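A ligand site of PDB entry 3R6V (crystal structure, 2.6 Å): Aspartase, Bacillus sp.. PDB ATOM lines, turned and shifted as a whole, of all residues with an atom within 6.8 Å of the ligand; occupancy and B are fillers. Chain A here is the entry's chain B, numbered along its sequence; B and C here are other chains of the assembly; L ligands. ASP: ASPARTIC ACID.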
ATOM      1  N   GLY A  98      21.908  -2.670  10.648  1.00  0.00           N
ATOM      2  CA  GLY A  98      20.742  -2.379  11.461  1.00  0.00           C
ATOM      3  C   GLY A  98      20.188  -0.987  11.237  1.00  0.00           C
ATOM      4  O   GLY A  98      19.281  -0.561  11.953  1.00  0.00           O
ATOM      5  N   ALA A  99      20.743  -0.293  10.247  1.00  0.00           N
ATOM      6  CA  ALA A  99      20.197   0.980   9.788  1.00  0.00           C
ATOM      7  C   ALA A  99      20.072   2.085  10.856  1.00  0.00           C
ATOM      8  O   ALA A  99      19.191   2.940  10.766  1.00  0.00           O
ATOM      9  CB  ALA A  99      18.837   0.739   9.113  1.00  0.00           C
ATOM     10  N   GLY A 100      20.956   2.060  11.857  1.00  0.00           N
ATOM     11  CA  GLY A 100      20.952   3.055  12.922  1.00  0.00           C
ATOM     12  C   GLY A 100      20.242   2.612  14.197  1.00  0.00           C
ATOM     13  O   GLY A 100      20.221   3.360  15.186  1.00  0.00           O
ATOM     14  N   THR A 101      19.666   1.406  14.195  1.00  0.00           N
ATOM     15  CA  THR A 101      18.964   0.910  15.377  1.00  0.00           C
ATOM     16  C   THR A 101      19.885   0.972  16.584  1.00  0.00           C
ATOM     17  O   THR A 101      19.469   1.386  17.678  1.00  0.00           O
ATOM     18  CB  THR A 101      18.378  -0.515  15.185  1.00  0.00           C
ATOM     19  OG1 THR A 101      17.232  -0.425  14.350  1.00  0.00           O
ATOM     20  CG2 THR A 101      17.914  -1.093  16.492  1.00  0.00           C
ATOM     21  N   ASN A 104      20.374   4.522  17.748  1.00  0.00           N
ATOM     22  CA  ASN A 104      19.135   4.896  18.412  1.00  0.00           C
ATOM     23  C   ASN A 104      19.025   4.280  19.809  1.00  0.00           C
ATOM     24  O   ASN A 104      18.752   4.993  20.789  1.00  0.00           O
ATOM     25  CB  ASN A 104      17.942   4.491  17.540  1.00  0.00           C
ATOM     26  CG  ASN A 104      16.632   4.998  18.084  1.00  0.00           C
ATOM     27  OD1 ASN A 104      16.523   6.153  18.546  1.00  0.00           O
ATOM     28  ND2 ASN A 104      15.601   4.156  18.020  1.00  0.00           N
ATOM     29  N   MET A 105      19.282   2.970  19.910  1.00  0.00           N
ATOM     30  CA  MET A 105      19.253   2.254  21.189  1.00  0.00           C
ATOM     31  C   MET A 105      20.359   2.687  22.140  1.00  0.00           C
ATOM     32  O   MET A 105      20.173   2.670  23.353  1.00  0.00           O
ATOM     33  CB  MET A 105      19.297   0.748  20.978  1.00  0.00           C
ATOM     34  CG  MET A 105      18.001   0.132  20.436  1.00  0.00           C
ATOM     35  SD  MET A 105      16.449   0.677  21.214  1.00  0.00           S
ATOM     36  CE  MET A 105      16.682   0.227  22.947  1.00  0.00           C
ATOM     37  N   ASN A 136      11.863   5.716  23.933  1.00  0.00           N
ATOM     38  CA  ASN A 136      11.623   5.572  22.493  1.00  0.00           C
ATOM     39  C   ASN A 136      10.127   5.476  22.182  1.00  0.00           C
ATOM     40  O   ASN A 136       9.722   5.011  21.106  1.00  0.00           O
ATOM     41  CB  ASN A 136      12.363   4.332  21.971  1.00  0.00           C
ATOM     42  CG  ASN A 136      12.610   4.366  20.469  1.00  0.00           C
ATOM     43  OD1 ASN A 136      13.401   5.161  19.971  1.00  0.00           O
ATOM     44  ND2 ASN A 136      11.944   3.459  19.737  1.00  0.00           N
ATOM     45  N   GLN A 139       7.999   6.711  18.773  1.00  0.00           N
ATOM     46  CA  GLN A 139       8.977   6.917  17.730  1.00  0.00           C
ATOM     47  C   GLN A 139       9.643   5.604  17.307  1.00  0.00           C
ATOM     48  O   GLN A 139       9.662   4.622  18.057  1.00  0.00           O
ATOM     49  CB  GLN A 139      10.011   7.963  18.180  1.00  0.00           C
ATOM     50  CG  GLN A 139      11.069   7.448  19.139  1.00  0.00           C
ATOM     51  CD  GLN A 139      11.581   8.515  20.095  1.00  0.00           C
ATOM     52  OE1 GLN A 139      12.678   9.048  19.914  1.00  0.00           O
ATOM     53  NE2 GLN A 139      10.802   8.813  21.133  1.00  0.00           N
ATOM     54  N   SER A 140      10.196   5.610  16.099  1.00  0.00           N
ATOM     55  CA  SER A 140      10.885   4.476  15.526  1.00  0.00           C
ATOM     56  C   SER A 140      12.351   4.837  15.391  1.00  0.00           C
ATOM     57  O   SER A 140      12.722   5.979  15.651  1.00  0.00           O
ATOM     58  CB  SER A 140      10.297   4.199  14.149  1.00  0.00           C
ATOM     59  OG  SER A 140      11.194   3.470  13.325  1.00  0.00           O
ATOM     60  N   THR A 141      13.182   3.874  14.982  1.00  0.00           N
ATOM     61  CA  THR A 141      14.531   4.192  14.524  1.00  0.00           C
ATOM     62  C   THR A 141      14.423   5.016  13.242  1.00  0.00           C
ATOM     63  O   THR A 141      15.202   5.949  13.021  1.00  0.00           O
ATOM     64  CB  THR A 141      15.331   2.929  14.195  1.00  0.00           C
ATOM     65  OG1 THR A 141      15.444   2.111  15.364  1.00  0.00           O
ATOM     66  CG2 THR A 141      16.730   3.260  13.707  1.00  0.00           C
ATOM     67  N   ASN A 142      13.436   4.670  12.429  1.00  0.00           N
ATOM     68  CA  ASN A 142      13.312   5.173  11.062  1.00  0.00           C
ATOM     69  C   ASN A 142      12.793   6.605  10.943  1.00  0.00           C
ATOM     70  O   ASN A 142      12.661   7.126   9.842  1.00  0.00           O
ATOM     71  CB  ASN A 142      12.489   4.191  10.210  1.00  0.00           C
ATOM     72  CG  ASN A 142      13.048   2.771  10.249  1.00  0.00           C
ATOM     73  OD1 ASN A 142      14.233   2.545  10.515  1.00  0.00           O
ATOM     74  ND2 ASN A 142      12.184   1.801   9.988  1.00  0.00           N
ATOM     75  N   ALA A 231       7.486   3.182  11.485  1.00  0.00           N
ATOM     76  CA  ALA A 231       8.449   2.325  10.802  1.00  0.00           C
ATOM     77  C   ALA A 231       8.609   2.579   9.305  1.00  0.00           C
ATOM     78  O   ALA A 231       9.656   2.274   8.722  1.00  0.00           O
ATOM     79  CB  ALA A 231       8.120   0.839  11.057  1.00  0.00           C
ATOM     80  N   VAL A 232       7.584   3.154   8.676  1.00  0.00           N
ATOM     81  CA  VAL A 232       7.465   3.124   7.230  1.00  0.00           C
ATOM     82  C   VAL A 232       6.969   4.456   6.648  1.00  0.00           C
ATOM     83  O   VAL A 232       6.977   4.665   5.439  1.00  0.00           O
ATOM     84  CB  VAL A 232       6.566   1.933   6.835  1.00  0.00           C
ATOM     85  CG1 VAL A 232       5.683   2.228   5.648  1.00  0.00           C
ATOM     86  CG2 VAL A 232       7.411   0.682   6.629  1.00  0.00           C
ATOM     87  N   LEU A 358      12.769   1.581   3.351  1.00  0.00           N
ATOM     88  CA  LEU A 358      13.938   2.044   4.105  1.00  0.00           C
ATOM     89  C   LEU A 358      15.233   1.854   3.316  1.00  0.00           C
ATOM     90  O   LEU A 358      15.403   0.845   2.635  1.00  0.00           O
ATOM     91  CB  LEU A 358      14.041   1.290   5.438  1.00  0.00           C
ATOM     92  CG  LEU A 358      15.113   1.727   6.447  1.00  0.00           C
ATOM     93  CD1 LEU A 358      14.849   3.163   6.980  1.00  0.00           C
ATOM     94  CD2 LEU A 358      15.248   0.691   7.582  1.00  0.00           C
ATOM     95  N   VAL A 360      18.756   1.025   4.255  1.00  0.00           N
ATOM     96  CA  VAL A 360      19.493   0.559   5.433  1.00  0.00           C
ATOM     97  C   VAL A 360      20.994   0.902   5.414  1.00  0.00           C
ATOM     98  O   VAL A 360      21.733   0.514   6.305  1.00  0.00           O
ATOM     99  CB  VAL A 360      19.314  -0.964   5.658  1.00  0.00           C
ATOM    100  CG1 VAL A 360      17.827  -1.309   5.817  1.00  0.00           C
ATOM    101  CG2 VAL A 360      19.946  -1.785   4.532  1.00  0.00           C
ATOM    102  N   PRO B 316      18.199  -7.409  18.408  1.00  0.00           N
ATOM    103  CA  PRO B 316      16.821  -7.000  18.099  1.00  0.00           C
ATOM    104  C   PRO B 316      16.810  -6.062  16.877  1.00  0.00           C
ATOM    105  O   PRO B 316      17.598  -5.103  16.797  1.00  0.00           O
ATOM    106  CB  PRO B 316      16.360  -6.298  19.374  1.00  0.00           C
ATOM    107  CG  PRO B 316      17.216  -6.907  20.468  1.00  0.00           C
ATOM    108  CD  PRO B 316      18.541  -7.153  19.826  1.00  0.00           C
ATOM    109  N   GLY B 317      15.937  -6.369  15.908  1.00  0.00           N
ATOM    110  CA  GLY B 317      15.872  -5.603  14.658  1.00  0.00           C
ATOM    111  C   GLY B 317      15.079  -4.306  14.740  1.00  0.00           C
ATOM    112  O   GLY B 317      15.471  -3.294  14.149  1.00  0.00           O
ATOM    113  N   SER B 318      13.953  -4.336  15.455  1.00  0.00           N
ATOM    114  CA  SER B 318      13.073  -3.176  15.536  1.00  0.00           C
ATOM    115  C   SER B 318      12.865  -2.691  16.964  1.00  0.00           C
ATOM    116  O   SER B 318      12.669  -3.483  17.891  1.00  0.00           O
ATOM    117  CB  SER B 318      11.737  -3.455  14.867  1.00  0.00           C
ATOM    118  OG  SER B 318      11.029  -2.242  14.625  1.00  0.00           O
ATOM    119  N   SER B 319      12.902  -1.360  17.118  1.00  0.00           N
ATOM    120  CA  SER B 319      12.720  -0.697  18.407  1.00  0.00           C
ATOM    121  C   SER B 319      11.235  -0.497  18.765  1.00  0.00           C
ATOM    122  O   SER B 319      10.917  -0.216  19.932  1.00  0.00           O
ATOM    123  CB  SER B 319      13.463   0.633  18.425  1.00  0.00           C
ATOM    124  OG  SER B 319      12.977   1.498  17.405  1.00  0.00           O
ATOM    125  N   ILE B 320      10.354  -0.638  17.765  1.00  0.00           N
ATOM    126  CA  ILE B 320       8.888  -0.691  17.999  1.00  0.00           C
ATOM    127  C   ILE B 320       8.164  -1.985  17.549  1.00  0.00           C
ATOM    128  O   ILE B 320       6.937  -2.104  17.682  1.00  0.00           O
ATOM    129  CB  ILE B 320       8.111   0.616  17.537  1.00  0.00           C
ATOM    130  CG1 ILE B 320       8.367   0.942  16.051  1.00  0.00           C
ATOM    131  CG2 ILE B 320       8.394   1.789  18.509  1.00  0.00           C
ATOM    132  CD1 ILE B 320       7.264   1.811  15.415  1.00  0.00           C
ATOM    133  N   MET B 321       8.918  -2.954  17.012  1.00  0.00           N
ATOM    134  CA  MET B 321       8.392  -4.289  16.714  1.00  0.00           C
ATOM    135  C   MET B 321       9.333  -5.394  17.233  1.00  0.00           C
ATOM    136  O   MET B 321      10.286  -5.788  16.527  1.00  0.00           O
ATOM    137  CB  MET B 321       8.063  -4.444  15.221  1.00  0.00           C
ATOM    138  CG  MET B 321       7.381  -5.776  14.854  1.00  0.00           C
ATOM    139  SD  MET B 321       6.141  -5.673  13.518  1.00  0.00           S
ATOM    140  CE  MET B 321       7.009  -4.658  12.296  1.00  0.00           C
ATOM    141  N   LYS B 324      10.725  -9.065  14.330  1.00  0.00           N
ATOM    142  CA  LYS B 324      11.514  -9.337  13.085  1.00  0.00           C
ATOM    143  C   LYS B 324      13.053  -9.170  13.152  1.00  0.00           C
ATOM    144  O   LYS B 324      13.570  -8.234  13.771  1.00  0.00           O
ATOM    145  CB  LYS B 324      10.929  -8.567  11.872  1.00  0.00           C
ATOM    146  CG  LYS B 324      10.499  -7.109  12.174  1.00  0.00           C
ATOM    147  CD  LYS B 324      11.399  -6.073  11.518  1.00  0.00           C
ATOM    148  CE  LYS B 324      10.764  -5.502  10.266  1.00  0.00           C
ATOM    149  NZ  LYS B 324      11.811  -4.966   9.359  1.00  0.00           N
ATOM    150  N   ASN B 326      16.469  -8.531  11.138  1.00  0.00           N
ATOM    151  CA  ASN B 326      17.081  -7.982   9.943  1.00  0.00           C
ATOM    152  C   ASN B 326      18.451  -8.603   9.694  1.00  0.00           C
ATOM    153  O   ASN B 326      19.126  -9.016  10.640  1.00  0.00           O
ATOM    154  CB  ASN B 326      17.183  -6.461  10.052  1.00  0.00           C
ATOM    155  CG  ASN B 326      15.886  -5.831  10.520  1.00  0.00           C
ATOM    156  OD1 ASN B 326      14.790  -6.171  10.036  1.00  0.00           O
ATOM    157  ND2 ASN B 326      15.986  -4.924  11.482  1.00  0.00           N
ATOM    158  N   ARG C 186       8.140  -3.132   3.518  1.00  0.00           N
ATOM    159  CA  ARG C 186       9.342  -3.921   3.796  1.00  0.00           C
ATOM    160  C   ARG C 186      10.467  -2.981   4.136  1.00  0.00           C
ATOM    161  O   ARG C 186      10.765  -2.049   3.391  1.00  0.00           O
ATOM    162  CB  ARG C 186       9.766  -4.735   2.571  1.00  0.00           C
ATOM    163  CG  ARG C 186       8.839  -5.869   2.212  1.00  0.00           C
ATOM    164  CD  ARG C 186       9.355  -6.610   0.977  1.00  0.00           C
ATOM    165  NE  ARG C 186       8.345  -7.509   0.419  1.00  0.00           N
ATOM    166  CZ  ARG C 186       7.419  -7.148  -0.474  1.00  0.00           C
ATOM    167  NH1 ARG C 186       7.362  -5.902  -0.933  1.00  0.00           N
ATOM    168  NH2 ARG C 186       6.545  -8.042  -0.907  1.00  0.00           N
ATOM    169  N   THR C 187      11.092  -3.231   5.275  1.00  0.00           N
ATOM    170  CA  THR C 187      12.308  -2.532   5.638  1.00  0.00           C
ATOM    171  C   THR C 187      13.341  -3.612   5.882  1.00  0.00           C
ATOM    172  O   THR C 187      13.020  -4.631   6.489  1.00  0.00           O
ATOM    173  CB  THR C 187      12.082  -1.681   6.894  1.00  0.00           C
ATOM    174  OG1 THR C 187      11.760  -2.538   8.000  1.00  0.00           O
ATOM    175  CG2 THR C 187      10.937  -0.693   6.684  1.00  0.00           C
ATOM    176  N   HIS C 188      14.569  -3.422   5.410  1.00  0.00           N
ATOM    177  CA  HIS C 188      15.600  -4.467   5.471  1.00  0.00           C
ATOM    178  C   HIS C 188      15.233  -5.679   4.618  1.00  0.00           C
ATOM    179  O   HIS C 188      15.854  -6.747   4.753  1.00  0.00           O
ATOM    180  CB  HIS C 188      15.853  -4.944   6.913  1.00  0.00           C
ATOM    181  CG  HIS C 188      16.221  -3.860   7.869  1.00  0.00           C
ATOM    182  ND1 HIS C 188      17.526  -3.583   8.218  1.00  0.00           N
ATOM    183  CD2 HIS C 188      15.453  -3.010   8.594  1.00  0.00           C
ATOM    184  CE1 HIS C 188      17.546  -2.603   9.094  1.00  0.00           C
ATOM    185  NE2 HIS C 188      16.302  -2.236   9.340  1.00  0.00           N
ATOM    186  N   GLN C 190      12.597  -7.105   5.118  1.00  0.00           N
ATOM    187  CA  GLN C 190      11.898  -7.885   6.138  1.00  0.00           C
ATOM    188  C   GLN C 190      10.490  -7.290   6.283  1.00  0.00           C
ATOM    189  O   GLN C 190      10.333  -6.054   6.254  1.00  0.00           O
ATOM    190  CB  GLN C 190      12.705  -7.787   7.441  1.00  0.00           C
ATOM    191  CG  GLN C 190      12.833  -9.047   8.293  1.00  0.00           C
ATOM    192  CD  GLN C 190      13.423 -10.235   7.578  1.00  0.00           C
ATOM    193  OE1 GLN C 190      14.319 -10.128   6.737  1.00  0.00           O
ATOM    194  NE2 GLN C 190      12.938 -11.411   7.935  1.00  0.00           N
ATOM    195  N   ASP C 191       9.473  -8.142   6.380  1.00  0.00           N
ATOM    196  CA  ASP C 191       8.060  -7.700   6.507  1.00  0.00           C
ATOM    197  C   ASP C 191       7.893  -6.701   7.646  1.00  0.00           C
ATOM    198  O   ASP C 191       8.357  -6.950   8.757  1.00  0.00           O
ATOM    199  CB  ASP C 191       7.113  -8.886   6.806  1.00  0.00           C
ATOM    200  CG  ASP C 191       7.191 -10.004   5.778  1.00  0.00           C
ATOM    201  OD1 ASP C 191       6.649 -11.097   6.064  1.00  0.00           O
ATOM    202  OD2 ASP C 191       7.789  -9.797   4.692  1.00  0.00           O
ATOM    203  N   ALA C 192       7.228  -5.579   7.366  1.00  0.00           N
ATOM    204  CA  ALA C 192       7.023  -4.540   8.370  1.00  0.00           C
ATOM    205  C   ALA C 192       5.524  -4.358   8.711  1.00  0.00           C
ATOM    206  O   ALA C 192       4.906  -5.213   9.358  1.00  0.00           O
ATOM    207  CB  ALA C 192       7.676  -3.241   7.926  1.00  0.00           C
HETATM  208  N   ASP L   1      15.273  -0.215  11.620  1.00  0.00           N
HETATM  209  CA  ASP L   1      14.060  -0.945  12.083  1.00  0.00           C
HETATM  210  C   ASP L   1      13.297  -1.590  10.940  1.00  0.00           C
HETATM  211  O   ASP L   1      12.907  -0.916   9.984  1.00  0.00           O
HETATM  212  CB  ASP L   1      13.105  -0.023  12.846  1.00  0.00           C
HETATM  213  CG  ASP L   1      13.516   0.204  14.280  1.00  0.00           C
HETATM  214  OD1 ASP L   1      12.836   0.994  14.967  1.00  0.00           O
HETATM  215  OD2 ASP L   1      14.540  -0.385  14.716  1.00  0.00           O
HETATM  216  OXT ASP L   1      13.031  -2.799  10.996  1.00  0.00           O
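OD1 of the ligand is in hydrogen-bond range of N of Thr 141. OD1 of the ligand lies within hydrogen-bond range of OG of Ser 140, 3.4 Å away. The side-chain hydroxyl (OG1) of Thr 187 of chain C lies within hydrogen-bond range of an oxygen (O) of the ligand, 2.8 Å away. The side-chain amide nitrogen (ND2) of Asn 142 is in hydrogen-bond range of an oxygen (O) of the ligand (2.8 Å). The side-chain hydroxyl of Thr 101 sits at hydrogen-bond distance from an oxygen (OD2) of the ligand (2.7 Å). The backbone NH (N) of Ser 319 of chain B sits at hydrogen-bond distance from an oxygen (OD2) of the ligand. OD2 of the ligand lies within hydrogen-bond range of OG1 of Thr 141 (2.7 Å). The side-chain amino group of Lys 324 of chain B is in salt-bridge range of an oxygen (OXT) of the ligand (3.0 Å). An oxygen (OD1) of the ligand sits at hydrogen-bond distance from the side-chain hydroxyl of Ser 319 of chain B (2.5 Å). NE2 of His 188 of chain C sits at hydrogen-bond distance from N of the ligand, 3.2 Å away.
The side-chain amide nitrogen of Asn 104 sits at hydrogen-bond distance from the side-chain hydroxyl of Thr 141. The side-chain hydroxyl (OG1) of Thr 187 of chain C is in hydrogen-bond range of the side-chain amino group (NZ) of Lys 324 of chain B, at 2.8 Å. The side-chain hydroxyl of Ser 140 lies within hydrogen-bond range of the backbone NH of Asn 142. The side-chain hydroxyl of Thr 101 sits at hydrogen-bond distance from the backbone carbonyl oxygen of Gly 317 of chain B (3.4 Å). The side-chain hydroxyl of Thr 101 is in hydrogen-bond range of the backbone carbonyl oxygen of Gly 98 (3.2 Å). The side-chain hydroxyl of Ser 319 of chain B sits at hydrogen-bond distance from the side-chain hydroxyl of Thr 141 (3.3 Å). The side-chain hydroxyl (OG) of Ser 318 of chain B is in hydrogen-bond range of the backbone NH (N) of Met 321 of chain B (3.3 Å). The side-chain amide nitrogen (ND2) of Asn 142 lies within hydrogen-bond range of the backbone carbonyl oxygen (O) of Ala 231, 2.9 Å away.
The backbone carbonyl oxygen (O) of Gly 317 of chain B sits close to an oxygen (OD2) of the ligand. Merely in contact with the ligand: Ser 318 of chain B (3.3 Å), Asn 326 of chain B (3.7 Å) and Leu 358 (3.7 Å). Hydrophobic or aromatic side chains that line the ligand: Leu 358 and His 188 of chain C.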
